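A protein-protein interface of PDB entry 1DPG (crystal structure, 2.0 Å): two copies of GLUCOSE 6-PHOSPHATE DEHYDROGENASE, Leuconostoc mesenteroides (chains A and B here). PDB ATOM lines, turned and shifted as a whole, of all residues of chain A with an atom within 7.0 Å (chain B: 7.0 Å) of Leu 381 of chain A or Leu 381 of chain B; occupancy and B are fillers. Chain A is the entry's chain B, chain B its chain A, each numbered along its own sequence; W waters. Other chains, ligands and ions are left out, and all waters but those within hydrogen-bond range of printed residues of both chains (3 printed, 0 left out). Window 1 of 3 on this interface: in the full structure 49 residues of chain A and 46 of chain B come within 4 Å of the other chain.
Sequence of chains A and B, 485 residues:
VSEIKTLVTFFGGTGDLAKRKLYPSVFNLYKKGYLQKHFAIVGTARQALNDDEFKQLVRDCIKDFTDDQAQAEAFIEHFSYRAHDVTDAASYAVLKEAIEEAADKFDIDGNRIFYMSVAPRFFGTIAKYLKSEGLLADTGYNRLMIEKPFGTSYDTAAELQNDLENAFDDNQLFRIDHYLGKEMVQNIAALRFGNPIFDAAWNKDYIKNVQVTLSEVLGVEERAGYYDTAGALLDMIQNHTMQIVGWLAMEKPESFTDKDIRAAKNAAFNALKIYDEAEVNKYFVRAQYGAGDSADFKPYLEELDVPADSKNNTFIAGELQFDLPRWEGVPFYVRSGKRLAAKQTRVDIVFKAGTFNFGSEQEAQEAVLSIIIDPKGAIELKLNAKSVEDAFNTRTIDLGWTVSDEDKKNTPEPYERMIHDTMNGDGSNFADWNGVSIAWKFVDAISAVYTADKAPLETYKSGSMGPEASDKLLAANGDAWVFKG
The backbone carbonyl oxygen of Gly 400 of chain A is in hydrogen-bond range of the backbone NH of Gly 400 of chain B, 2.8 Å away.
Water W1 lies within hydrogen-bond range of O of Ile 197 of chain A and O of Ile 197 of chain B. Water W3 bridges the backbone NH of Asp 398 of chain A and the indole nitrogen of Trp 401 of chain B. Water W2 bridges O of Gly 400 of chain A and O of Asp 398 of chain B.
Leu 381 of chain A touches its own counterpart, Leu 381 of chain B. Ile 397 of chain A touches Trp 401 of chain B, and with the chains exchanged Trp 401 of chain A touches Ile 397 of chain B. Leu 399 of chain A touches Trp 401 of chain B, and with the chains exchanged Trp 401 of chain A touches Leu 399 of chain B. Positions printed for both chains: 197, 198, 349, 351, 367, 368, 369, 370, 379, 380, 381, 382, 383, 397, 398, 399, 400 and 401.
Hydrophobic or aromatic side chains of chain B that line the printed part of chain A: Ile 197, Phe 198, Ile 379, Leu 381, Leu 383, Ile 397, Leu 399 and Trp 401. Hydrophobic or aromatic side chains of chain A within 4 Å of the printed part of chain B: Phe 198, Phe 351, Ile 379, Leu 381, Leu 383, Ile 397, Leu 399 and Trp 401. Among the printed residues, 21 pairs touch across the chains. Among the printed residues, no Asp or Glu carboxylate lies within 4 Å of a Lys or Arg side-chain nitrogen of the other chain.
Ile 197 of chain A touches none of the printed residues of chain B. Ser 370 of chain A touches none of the printed residues of chain B. Of the printed residues of chain B, Leu 381 of chain A touches Leu 381 and Leu 399. Printed residues of chain B within 4 Å of Asp 398 of chain A: Gly 400 and Trp 401. Printed residues of chain A within 4 Å of Phe 198 of chain B: Leu 383 (3.6 Å). Leu 381 of chain B touches one residue of chain A. The nearest printed residue of chain B that does not touch Leu 381 of chain A is Ile 197 of chain B (4.8 Å). The nearest residue of chain A that does not touch Leu 381 of chain B is Leu 399 of chain A (4.02 Å).
Leu 381 of chain A touches Leu 399 of chain B (CB to CD1, 3.99 Å). CE2 of Phe 198 of chain B touches CD1 of Leu 383 of chain A, 3.6 Å away. Ile 397 of chain A touches Trp 401 of chain B. Gly 400 of chain B touches Asp 398 of chain A (O to O, 3.7 Å). Leu 399 of chain A touches Leu 399 of chain B (CB to CB, 3.8 Å). Trp 401 of chain A touches Leu 399 of chain B (CB to CD2, 3.6 Å).
The backbone carbonyl oxygen of Ile 379 of chain A is in hydrogen-bond range of the backbone NH of Trp 401 of chain A (2.9 Å). The backbone carbonyl oxygen (O) of Leu 381 of chain A is in hydrogen-bond range of the backbone NH (N) of Leu 399 of chain A (2.8 Å). The backbone carbonyl oxygen (O) of Leu 383 of chain A is in hydrogen-bond range of the backbone NH (N) of Ile 397 of chain A, 2.8 Å away.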
ATOM      1  N   ILE A 197     -18.779 -14.723  14.401  1.00  0.00           N
ATOM      2  CA  ILE A 197     -17.529 -15.417  14.141  1.00  0.00           C
ATOM      3  C   ILE A 197     -17.727 -16.567  13.164  1.00  0.00           C
ATOM      4  O   ILE A 197     -16.807 -16.917  12.453  1.00  0.00           O
ATOM      5  CB  ILE A 197     -16.851 -15.948  15.439  1.00  0.00           C
ATOM      6  CG1 ILE A 197     -17.801 -16.860  16.209  1.00  0.00           C
ATOM      7  CG2 ILE A 197     -16.442 -14.781  16.323  1.00  0.00           C
ATOM      8  CD1 ILE A 197     -17.164 -17.508  17.447  1.00  0.00           C
ATOM      9  N   PHE A 198     -18.908 -17.181  13.162  1.00  0.00           N
ATOM     10  CA  PHE A 198     -19.188 -18.274  12.228  1.00  0.00           C
ATOM     11  C   PHE A 198     -19.829 -17.749  10.930  1.00  0.00           C
ATOM     12  O   PHE A 198     -19.485 -18.175   9.815  1.00  0.00           O
ATOM     13  CB  PHE A 198     -20.069 -19.314  12.900  1.00  0.00           C
ATOM     14  CG  PHE A 198     -19.330 -20.167  13.881  1.00  0.00           C
ATOM     15  CD1 PHE A 198     -18.075 -20.669  13.572  1.00  0.00           C
ATOM     16  CD2 PHE A 198     -19.876 -20.458  15.114  1.00  0.00           C
ATOM     17  CE1 PHE A 198     -17.375 -21.444  14.483  1.00  0.00           C
ATOM     18  CE2 PHE A 198     -19.187 -21.227  16.026  1.00  0.00           C
ATOM     19  CZ  PHE A 198     -17.935 -21.721  15.706  1.00  0.00           C
ATOM     20  N   ILE A 349     -17.743 -29.506   9.251  1.00  0.00           N
ATOM     21  CA  ILE A 349     -17.256 -28.407   8.440  1.00  0.00           C
ATOM     22  C   ILE A 349     -15.781 -28.275   8.766  1.00  0.00           C
ATOM     23  O   ILE A 349     -15.415 -28.026   9.912  1.00  0.00           O
ATOM     24  CB  ILE A 349     -18.009 -27.154   8.799  1.00  0.00           C
ATOM     25  CG1 ILE A 349     -19.490 -27.383   8.487  1.00  0.00           C
ATOM     26  CG2 ILE A 349     -17.435 -25.974   8.063  1.00  0.00           C
ATOM     27  CD1 ILE A 349     -20.417 -26.437   9.170  1.00  0.00           C
ATOM     28  N   PHE A 351     -12.289 -26.467   8.495  1.00  0.00           N
ATOM     29  CA  PHE A 351     -11.712 -25.140   8.265  1.00  0.00           C
ATOM     30  C   PHE A 351     -10.264 -25.224   7.786  1.00  0.00           C
ATOM     31  O   PHE A 351      -9.513 -26.071   8.245  1.00  0.00           O
ATOM     32  CB  PHE A 351     -11.762 -24.322   9.554  1.00  0.00           C
ATOM     33  CG  PHE A 351     -13.149 -23.921   9.961  1.00  0.00           C
ATOM     34  CD1 PHE A 351     -13.786 -22.843   9.336  1.00  0.00           C
ATOM     35  CD2 PHE A 351     -13.827 -24.620  10.955  1.00  0.00           C
ATOM     36  CE1 PHE A 351     -15.075 -22.465   9.689  1.00  0.00           C
ATOM     37  CE2 PHE A 351     -15.134 -24.257  11.327  1.00  0.00           C
ATOM     38  CZ  PHE A 351     -15.761 -23.168  10.688  1.00  0.00           C
ATOM     39  N   ALA A 367      -9.220 -26.641  12.003  1.00  0.00           N
ATOM     40  CA  ALA A 367     -10.239 -26.671  13.037  1.00  0.00           C
ATOM     41  C   ALA A 367     -11.461 -27.354  12.395  1.00  0.00           C
ATOM     42  O   ALA A 367     -11.629 -27.323  11.169  1.00  0.00           O
ATOM     43  CB  ALA A 367     -10.578 -25.268  13.470  1.00  0.00           C
ATOM     44  N   VAL A 368     -12.310 -27.976  13.197  1.00  0.00           N
ATOM     45  CA  VAL A 368     -13.480 -28.654  12.653  1.00  0.00           C
ATOM     46  C   VAL A 368     -14.693 -28.403  13.538  1.00  0.00           C
ATOM     47  O   VAL A 368     -14.607 -28.518  14.778  1.00  0.00           O
ATOM     48  CB  VAL A 368     -13.282 -30.180  12.616  1.00  0.00           C
ATOM     49  CG1 VAL A 368     -14.521 -30.864  12.039  1.00  0.00           C
ATOM     50  CG2 VAL A 368     -12.041 -30.551  11.858  1.00  0.00           C
ATOM     51  N   LEU A 369     -15.806 -28.041  12.906  1.00  0.00           N
ATOM     52  CA  LEU A 369     -17.065 -27.836  13.607  1.00  0.00           C
ATOM     53  C   LEU A 369     -17.965 -29.007  13.196  1.00  0.00           C
ATOM     54  O   LEU A 369     -18.229 -29.211  11.999  1.00  0.00           O
ATOM     55  CB  LEU A 369     -17.709 -26.526  13.161  1.00  0.00           C
ATOM     56  CG  LEU A 369     -19.131 -26.282  13.652  1.00  0.00           C
ATOM     57  CD1 LEU A 369     -19.128 -26.119  15.154  1.00  0.00           C
ATOM     58  CD2 LEU A 369     -19.698 -25.039  12.993  1.00  0.00           C
ATOM     59  N   SER A 370     -18.385 -29.809  14.166  1.00  0.00           N
ATOM     60  CA  SER A 370     -19.259 -30.942  13.890  1.00  0.00           C
ATOM     61  C   SER A 370     -20.648 -30.752  14.480  1.00  0.00           C
ATOM     62  O   SER A 370     -20.788 -30.357  15.637  1.00  0.00           O
ATOM     63  CB  SER A 370     -18.684 -32.222  14.498  1.00  0.00           C
ATOM     64  OG  SER A 370     -17.439 -32.560  13.922  1.00  0.00           O
ATOM     65  N   ILE A 379     -22.768 -30.892  19.525  1.00  0.00           N
ATOM     66  CA  ILE A 379     -22.013 -29.921  18.728  1.00  0.00           C
ATOM     67  C   ILE A 379     -20.583 -29.953  19.267  1.00  0.00           C
ATOM     68  O   ILE A 379     -20.372 -29.859  20.473  1.00  0.00           O
ATOM     69  CB  ILE A 379     -22.556 -28.500  18.889  1.00  0.00           C
ATOM     70  CG1 ILE A 379     -23.998 -28.436  18.392  1.00  0.00           C
ATOM     71  CG2 ILE A 379     -21.687 -27.514  18.137  1.00  0.00           C
ATOM     72  CD1 ILE A 379     -24.625 -27.078  18.552  1.00  0.00           C
ATOM     73  N   GLU A 380     -19.620 -30.173  18.384  1.00  0.00           N
ATOM     74  CA  GLU A 380     -18.227 -30.219  18.776  1.00  0.00           C
ATOM     75  C   GLU A 380     -17.410 -29.292  17.921  1.00  0.00           C
ATOM     76  O   GLU A 380     -17.686 -29.119  16.732  1.00  0.00           O
ATOM     77  CB  GLU A 380     -17.676 -31.626  18.649  1.00  0.00           C
ATOM     78  CG  GLU A 380     -18.181 -32.548  19.717  1.00  0.00           C
ATOM     79  CD  GLU A 380     -17.802 -33.990  19.457  1.00  0.00           C
ATOM     80  OE1 GLU A 380     -16.817 -34.226  18.711  1.00  0.00           O
ATOM     81  OE2 GLU A 380     -18.497 -34.887  19.996  1.00  0.00           O
ATOM     82  N   LEU A 381     -16.381 -28.727  18.536  1.00  0.00           N
ATOM     83  CA  LEU A 381     -15.481 -27.822  17.866  1.00  0.00           C
ATOM     84  C   LEU A 381     -14.058 -28.225  18.241  1.00  0.00           C
ATOM     85  O   LEU A 381     -13.667 -28.179  19.427  1.00  0.00           O
ATOM     86  CB  LEU A 381     -15.790 -26.386  18.291  1.00  0.00           C
ATOM     87  CG  LEU A 381     -14.970 -25.291  17.610  1.00  0.00           C
ATOM     88  CD1 LEU A 381     -15.131 -25.359  16.086  1.00  0.00           C
ATOM     89  CD2 LEU A 381     -15.406 -23.940  18.162  1.00  0.00           C
ATOM     90  N   LYS A 382     -13.356 -28.787  17.262  1.00  0.00           N
ATOM     91  CA  LYS A 382     -11.960 -29.188  17.425  1.00  0.00           C
ATOM     92  C   LYS A 382     -11.152 -27.911  17.121  1.00  0.00           C
ATOM     93  O   LYS A 382     -11.277 -27.348  16.026  1.00  0.00           O
ATOM     94  CB  LYS A 382     -11.609 -30.299  16.417  1.00  0.00           C
ATOM     95  CG  LYS A 382     -10.164 -30.736  16.477  1.00  0.00           C
ATOM     96  CD  LYS A 382      -9.749 -31.632  15.318  1.00  0.00           C
ATOM     97  CE  LYS A 382     -10.590 -32.892  15.249  1.00  0.00           C
ATOM     98  NZ  LYS A 382     -10.446 -33.742  16.471  1.00  0.00           N
ATOM     99  N   LEU A 383     -10.367 -27.435  18.089  1.00  0.00           N
ATOM    100  CA  LEU A 383      -9.569 -26.209  17.936  1.00  0.00           C
ATOM    101  C   LEU A 383      -8.122 -26.493  18.236  1.00  0.00           C
ATOM    102  O   LEU A 383      -7.808 -27.483  18.895  1.00  0.00           O
ATOM    103  CB  LEU A 383     -10.001 -25.157  18.958  1.00  0.00           C
ATOM    104  CG  LEU A 383     -11.342 -24.476  18.812  1.00  0.00           C
ATOM    105  CD1 LEU A 383     -11.525 -23.525  19.972  1.00  0.00           C
ATOM    106  CD2 LEU A 383     -11.418 -23.746  17.462  1.00  0.00           C
ATOM    107  N   ILE A 397      -7.751 -29.803  20.468  1.00  0.00           N
ATOM    108  CA  ILE A 397      -8.531 -30.174  21.633  1.00  0.00           C
ATOM    109  C   ILE A 397      -9.965 -30.045  21.145  1.00  0.00           C
ATOM    110  O   ILE A 397     -10.235 -29.326  20.174  1.00  0.00           O
ATOM    111  CB  ILE A 397      -8.258 -29.222  22.851  1.00  0.00           C
ATOM    112  CG1 ILE A 397      -8.550 -27.767  22.483  1.00  0.00           C
ATOM    113  CG2 ILE A 397      -6.800 -29.264  23.192  1.00  0.00           C
ATOM    114  CD1 ILE A 397      -8.565 -26.820  23.666  1.00  0.00           C
ATOM    115  N   ASP A 398     -10.880 -30.705  21.831  1.00  0.00           N
ATOM    116  CA  ASP A 398     -12.279 -30.688  21.446  1.00  0.00           C
ATOM    117  C   ASP A 398     -13.208 -30.063  22.481  1.00  0.00           C
ATOM    118  O   ASP A 398     -13.267 -30.522  23.616  1.00  0.00           O
ATOM    119  CB  ASP A 398     -12.762 -32.130  21.181  1.00  0.00           C
ATOM    120  CG  ASP A 398     -11.926 -32.857  20.125  1.00  0.00           C
ATOM    121  OD1 ASP A 398     -11.761 -32.326  19.008  1.00  0.00           O
ATOM    122  OD2 ASP A 398     -11.421 -33.967  20.416  1.00  0.00           O
ATOM    123  N   LEU A 399     -13.901 -28.996  22.106  1.00  0.00           N
ATOM    124  CA  LEU A 399     -14.871 -28.402  23.001  1.00  0.00           C
ATOM    125  C   LEU A 399     -16.167 -29.073  22.541  1.00  0.00           C
ATOM    126  O   LEU A 399     -16.425 -29.172  21.338  1.00  0.00           O
ATOM    127  CB  LEU A 399     -15.007 -26.907  22.776  1.00  0.00           C
ATOM    128  CG  LEU A 399     -13.779 -26.023  22.550  1.00  0.00           C
ATOM    129  CD1 LEU A 399     -14.145 -24.603  22.981  1.00  0.00           C
ATOM    130  CD2 LEU A 399     -12.581 -26.518  23.306  1.00  0.00           C
ATOM    131  N   GLY A 400     -16.984 -29.528  23.477  1.00  0.00           N
ATOM    132  CA  GLY A 400     -18.216 -30.178  23.091  1.00  0.00           C
ATOM    133  C   GLY A 400     -19.415 -29.773  23.917  1.00  0.00           C
ATOM    134  O   GLY A 400     -19.290 -29.170  24.992  1.00  0.00           O
ATOM    135  N   TRP A 401     -20.583 -30.114  23.400  1.00  0.00           N
ATOM    136  CA  TRP A 401     -21.854 -29.851  24.053  1.00  0.00           C
ATOM    137  C   TRP A 401     -22.774 -30.963  23.560  1.00  0.00           C
ATOM    138  O   TRP A 401     -22.581 -31.457  22.451  1.00  0.00           O
ATOM    139  CB  TRP A 401     -22.397 -28.485  23.624  1.00  0.00           C
ATOM    140  CG  TRP A 401     -23.857 -28.270  23.951  1.00  0.00           C
ATOM    141  CD1 TRP A 401     -24.383 -27.657  25.062  1.00  0.00           C
ATOM    142  CD2 TRP A 401     -24.975 -28.690  23.165  1.00  0.00           C
ATOM    143  NE1 TRP A 401     -25.762 -27.674  25.014  1.00  0.00           N
ATOM    144  CE2 TRP A 401     -26.151 -28.304  23.861  1.00  0.00           C
ATOM    145  CE3 TRP A 401     -25.101 -29.361  21.941  1.00  0.00           C
ATOM    146  CZ2 TRP A 401     -27.435 -28.569  23.367  1.00  0.00           C
ATOM    147  CZ3 TRP A 401     -26.370 -29.623  21.457  1.00  0.00           C
ATOM    148  CH2 TRP A 401     -27.522 -29.227  22.169  1.00  0.00           C
ATOM    149  N   ILE B 197     -10.387 -18.490  12.519  1.00  0.00           N
ATOM    150  CA  ILE B 197     -11.677 -17.934  12.904  1.00  0.00           C
ATOM    151  C   ILE B 197     -11.560 -16.993  14.101  1.00  0.00           C
ATOM    152  O   ILE B 197     -12.320 -16.030  14.198  1.00  0.00           O
ATOM    153  CB  ILE B 197     -12.804 -19.006  13.133  1.00  0.00           C
ATOM    154  CG1 ILE B 197     -12.367 -20.097  14.106  1.00  0.00           C
ATOM    155  CG2 ILE B 197     -13.202 -19.652  11.818  1.00  0.00           C
ATOM    156  CD1 ILE B 197     -13.418 -21.210  14.251  1.00  0.00           C
ATOM    157  N   PHE B 198     -10.624 -17.262  15.008  1.00  0.00           N
ATOM    158  CA  PHE B 198     -10.427 -16.376  16.157  1.00  0.00           C
ATOM    159  C   PHE B 198      -9.452 -15.264  15.784  1.00  0.00           C
ATOM    160  O   PHE B 198      -9.680 -14.089  16.082  1.00  0.00           O
ATOM    161  CB  PHE B 198      -9.919 -17.161  17.387  1.00  0.00           C
ATOM    162  CG  PHE B 198     -10.975 -18.021  18.013  1.00  0.00           C
ATOM    163  CD1 PHE B 198     -12.251 -17.518  18.235  1.00  0.00           C
ATOM    164  CD2 PHE B 198     -10.726 -19.337  18.328  1.00  0.00           C
ATOM    165  CE1 PHE B 198     -13.283 -18.333  18.767  1.00  0.00           C
ATOM    166  CE2 PHE B 198     -11.739 -20.146  18.853  1.00  0.00           C
ATOM    167  CZ  PHE B 198     -13.024 -19.634  19.069  1.00  0.00           C
ATOM    168  N   ILE B 349     -13.724 -13.257  26.808  1.00  0.00           N
ATOM    169  CA  ILE B 349     -13.807 -12.373  25.652  1.00  0.00           C
ATOM    170  C   ILE B 349     -15.271 -12.379  25.191  1.00  0.00           C
ATOM    171  O   ILE B 349     -15.844 -13.436  24.888  1.00  0.00           O
ATOM    172  CB  ILE B 349     -12.867 -12.858  24.556  1.00  0.00           C
ATOM    173  CG1 ILE B 349     -11.430 -12.685  25.040  1.00  0.00           C
ATOM    174  CG2 ILE B 349     -13.089 -12.069  23.285  1.00  0.00           C
ATOM    175  CD1 ILE B 349     -10.596 -13.883  24.866  1.00  0.00           C
ATOM    176  N   PHE B 351     -17.991 -11.242  22.661  1.00  0.00           N
ATOM    177  CA  PHE B 351     -18.135 -10.819  21.269  1.00  0.00           C
ATOM    178  C   PHE B 351     -19.435 -10.071  21.054  1.00  0.00           C
ATOM    179  O   PHE B 351     -20.449 -10.412  21.666  1.00  0.00           O
ATOM    180  CB  PHE B 351     -18.144 -12.031  20.361  1.00  0.00           C
ATOM    181  CG  PHE B 351     -16.890 -12.808  20.385  1.00  0.00           C
ATOM    182  CD1 PHE B 351     -15.771 -12.350  19.698  1.00  0.00           C
ATOM    183  CD2 PHE B 351     -16.826 -14.030  21.057  1.00  0.00           C
ATOM    184  CE1 PHE B 351     -14.591 -13.103  19.671  1.00  0.00           C
ATOM    185  CE2 PHE B 351     -15.655 -14.794  21.038  1.00  0.00           C
ATOM    186  CZ  PHE B 351     -14.531 -14.329  20.341  1.00  0.00           C
ATOM    187  N   ALA B 367     -21.688 -13.836  22.093  1.00  0.00           N
ATOM    188  CA  ALA B 367     -20.964 -15.096  22.273  1.00  0.00           C
ATOM    189  C   ALA B 367     -19.799 -14.794  23.247  1.00  0.00           C
ATOM    190  O   ALA B 367     -19.352 -13.638  23.337  1.00  0.00           O
ATOM    191  CB  ALA B 367     -20.412 -15.588  20.938  1.00  0.00           C
ATOM    192  N   VAL B 368     -19.295 -15.811  23.954  1.00  0.00           N
ATOM    193  CA  VAL B 368     -18.173 -15.609  24.894  1.00  0.00           C
ATOM    194  C   VAL B 368     -17.110 -16.705  24.874  1.00  0.00           C
ATOM    195  O   VAL B 368     -17.421 -17.898  24.964  1.00  0.00           O
ATOM    196  CB  VAL B 368     -18.650 -15.476  26.374  1.00  0.00           C
ATOM    197  CG1 VAL B 368     -17.459 -15.150  27.274  1.00  0.00           C
ATOM    198  CG2 VAL B 368     -19.711 -14.387  26.508  1.00  0.00           C
ATOM    199  N   LEU B 369     -15.858 -16.309  24.662  1.00  0.00           N
ATOM    200  CA  LEU B 369     -14.772 -17.278  24.721  1.00  0.00           C
ATOM    201  C   LEU B 369     -14.169 -17.103  26.139  1.00  0.00           C
ATOM    202  O   LEU B 369     -13.772 -15.997  26.519  1.00  0.00           O
ATOM    203  CB  LEU B 369     -13.715 -16.988  23.656  1.00  0.00           C
ATOM    204  CG  LEU B 369     -12.489 -17.885  23.760  1.00  0.00           C
ATOM    205  CD1 LEU B 369     -12.863 -19.357  23.633  1.00  0.00           C
ATOM    206  CD2 LEU B 369     -11.518 -17.480  22.691  1.00  0.00           C
ATOM    207  N   SER B 370     -14.147 -18.167  26.931  1.00  0.00           N
ATOM    208  CA  SER B 370     -13.602 -18.101  28.283  1.00  0.00           C
ATOM    209  C   SER B 370     -12.441 -19.065  28.476  1.00  0.00           C
ATOM    210  O   SER B 370     -12.543 -20.240  28.130  1.00  0.00           O
ATOM    211  CB  SER B 370     -14.676 -18.441  29.299  1.00  0.00           C
ATOM    212  OG  SER B 370     -15.805 -17.615  29.124  1.00  0.00           O
ATOM    213  N   ILE B 379     -11.518 -24.417  28.903  1.00  0.00           N
ATOM    214  CA  ILE B 379     -11.833 -23.456  27.842  1.00  0.00           C
ATOM    215  C   ILE B 379     -13.292 -23.665  27.488  1.00  0.00           C
ATOM    216  O   ILE B 379     -13.721 -24.814  27.295  1.00  0.00           O
ATOM    217  CB  ILE B 379     -11.011 -23.700  26.564  1.00  0.00           C
ATOM    218  CG1 ILE B 379      -9.526 -23.564  26.854  1.00  0.00           C
ATOM    219  CG2 ILE B 379     -11.430 -22.719  25.449  1.00  0.00           C
ATOM    220  CD1 ILE B 379      -8.662 -23.780  25.632  1.00  0.00           C
ATOM    221  N   GLU B 380     -14.080 -22.595  27.528  1.00  0.00           N
ATOM    222  CA  GLU B 380     -15.468 -22.711  27.135  1.00  0.00           C
ATOM    223  C   GLU B 380     -15.942 -21.630  26.177  1.00  0.00           C
ATOM    224  O   GLU B 380     -15.473 -20.483  26.223  1.00  0.00           O
ATOM    225  CB  GLU B 380     -16.405 -22.902  28.315  1.00  0.00           C
ATOM    226  CG  GLU B 380     -16.274 -21.957  29.447  1.00  0.00           C
ATOM    227  CD  GLU B 380     -17.095 -22.435  30.645  1.00  0.00           C
ATOM    228  OE1 GLU B 380     -17.137 -23.668  30.876  1.00  0.00           O
ATOM    229  OE2 GLU B 380     -17.698 -21.588  31.350  1.00  0.00           O
ATOM    230  N   LEU B 381     -16.806 -22.042  25.250  1.00  0.00           N
ATOM    231  CA  LEU B 381     -17.331 -21.148  24.236  1.00  0.00           C
ATOM    232  C   LEU B 381     -18.858 -21.128  24.274  1.00  0.00           C
ATOM    233  O   LEU B 381     -19.507 -22.121  23.975  1.00  0.00           O
ATOM    234  CB  LEU B 381     -16.824 -21.605  22.876  1.00  0.00           C
ATOM    235  CG  LEU B 381     -17.204 -20.690  21.718  1.00  0.00           C
ATOM    236  CD1 LEU B 381     -16.592 -19.309  21.927  1.00  0.00           C
ATOM    237  CD2 LEU B 381     -16.712 -21.323  20.431  1.00  0.00           C
ATOM    238  N   LYS B 382     -19.412 -20.009  24.716  1.00  0.00           N
ATOM    239  CA  LYS B 382     -20.854 -19.819  24.824  1.00  0.00           C
ATOM    240  C   LYS B 382     -21.288 -19.368  23.445  1.00  0.00           C
ATOM    241  O   LYS B 382     -20.786 -18.357  22.954  1.00  0.00           O
ATOM    242  CB  LYS B 382     -21.138 -18.721  25.845  1.00  0.00           C
ATOM    243  CG  LYS B 382     -22.605 -18.480  26.102  1.00  0.00           C
ATOM    244  CD  LYS B 382     -22.834 -17.312  27.058  1.00  0.00           C
ATOM    245  CE  LYS B 382     -22.384 -17.654  28.470  1.00  0.00           C
ATOM    246  NZ  LYS B 382     -23.154 -18.795  29.041  1.00  0.00           N
ATOM    247  N   LEU B 383     -22.216 -20.105  22.830  1.00  0.00           N
ATOM    248  CA  LEU B 383     -22.687 -19.831  21.458  1.00  0.00           C
ATOM    249  C   LEU B 383     -24.207 -19.745  21.329  1.00  0.00           C
ATOM    250  O   LEU B 383     -24.936 -20.402  22.084  1.00  0.00           O
ATOM    251  CB  LEU B 383     -22.250 -20.980  20.531  1.00  0.00           C
ATOM    252  CG  LEU B 383     -20.799 -21.111  20.095  1.00  0.00           C
ATOM    253  CD1 LEU B 383     -20.608 -22.393  19.329  1.00  0.00           C
ATOM    254  CD2 LEU B 383     -20.408 -19.925  19.246  1.00  0.00           C
ATOM    255  N   ILE B 397     -25.791 -21.780  24.411  1.00  0.00           N
ATOM    256  CA  ILE B 397     -25.291 -23.057  24.919  1.00  0.00           C
ATOM    257  C   ILE B 397     -23.781 -22.929  25.152  1.00  0.00           C
ATOM    258  O   ILE B 397     -23.151 -22.021  24.614  1.00  0.00           O
ATOM    259  CB  ILE B 397     -25.563 -24.247  23.946  1.00  0.00           C
ATOM    260  CG1 ILE B 397     -24.819 -24.054  22.623  1.00  0.00           C
ATOM    261  CG2 ILE B 397     -27.073 -24.435  23.704  1.00  0.00           C
ATOM    262  CD1 ILE B 397     -25.016 -25.215  21.663  1.00  0.00           C
ATOM    263  N   ASP B 398     -23.190 -23.836  25.925  1.00  0.00           N
ATOM    264  CA  ASP B 398     -21.753 -23.762  26.213  1.00  0.00           C
ATOM    265  C   ASP B 398     -21.037 -24.999  25.758  1.00  0.00           C
ATOM    266  O   ASP B 398     -21.428 -26.088  26.159  1.00  0.00           O
ATOM    267  CB  ASP B 398     -21.496 -23.663  27.720  1.00  0.00           C
ATOM    268  CG  ASP B 398     -22.265 -22.541  28.374  1.00  0.00           C
ATOM    269  OD1 ASP B 398     -21.993 -21.357  28.079  1.00  0.00           O
ATOM    270  OD2 ASP B 398     -23.156 -22.850  29.188  1.00  0.00           O
ATOM    271  N   LEU B 399     -20.050 -24.854  24.879  1.00  0.00           N
ATOM    272  CA  LEU B 399     -19.240 -26.003  24.456  1.00  0.00           C
ATOM    273  C   LEU B 399     -18.099 -25.945  25.485  1.00  0.00           C
ATOM    274  O   LEU B 399     -17.593 -24.861  25.786  1.00  0.00           O
ATOM    275  CB  LEU B 399     -18.629 -25.807  23.065  1.00  0.00           C
ATOM    276  CG  LEU B 399     -19.445 -25.371  21.858  1.00  0.00           C
ATOM    277  CD1 LEU B 399     -18.994 -26.183  20.663  1.00  0.00           C
ATOM    278  CD2 LEU B 399     -20.934 -25.561  22.093  1.00  0.00           C
ATOM    279  N   GLY B 400     -17.660 -27.078  26.000  1.00  0.00           N
ATOM    280  CA  GLY B 400     -16.597 -27.020  26.976  1.00  0.00           C
ATOM    281  C   GLY B 400     -15.506 -28.037  26.787  1.00  0.00           C
ATOM    282  O   GLY B 400     -15.671 -29.023  26.059  1.00  0.00           O
ATOM    283  N   TRP B 401     -14.369 -27.747  27.413  1.00  0.00           N
ATOM    284  CA  TRP B 401     -13.189 -28.610  27.416  1.00  0.00           C
ATOM    285  C   TRP B 401     -12.416 -28.297  28.715  1.00  0.00           C
ATOM    286  O   TRP B 401     -12.325 -27.135  29.113  1.00  0.00           O
ATOM    287  CB  TRP B 401     -12.294 -28.295  26.221  1.00  0.00           C
ATOM    288  CG  TRP B 401     -10.977 -29.004  26.284  1.00  0.00           C
ATOM    289  CD1 TRP B 401     -10.688 -30.235  25.785  1.00  0.00           C
ATOM    290  CD2 TRP B 401      -9.780 -28.533  26.915  1.00  0.00           C
ATOM    291  NE1 TRP B 401      -9.390 -30.566  26.066  1.00  0.00           N
ATOM    292  CE2 TRP B 401      -8.807 -29.538  26.762  1.00  0.00           C
ATOM    293  CE3 TRP B 401      -9.442 -27.363  27.606  1.00  0.00           C
ATOM    294  CZ2 TRP B 401      -7.505 -29.414  27.279  1.00  0.00           C
ATOM    295  CZ3 TRP B 401      -8.150 -27.236  28.122  1.00  0.00           C
ATOM    296  CH2 TRP B 401      -7.202 -28.260  27.954  1.00  0.00           C
HETATM  297  O   HOH W   1     -14.400 -15.471  12.310  1.00  0.00           O
HETATM  298  O   HOH W   2     -20.649 -28.850  27.806  1.00  0.00           O
HETATM  299  O   HOH W   3      -9.688 -32.749  23.709  1.00  0.00           O
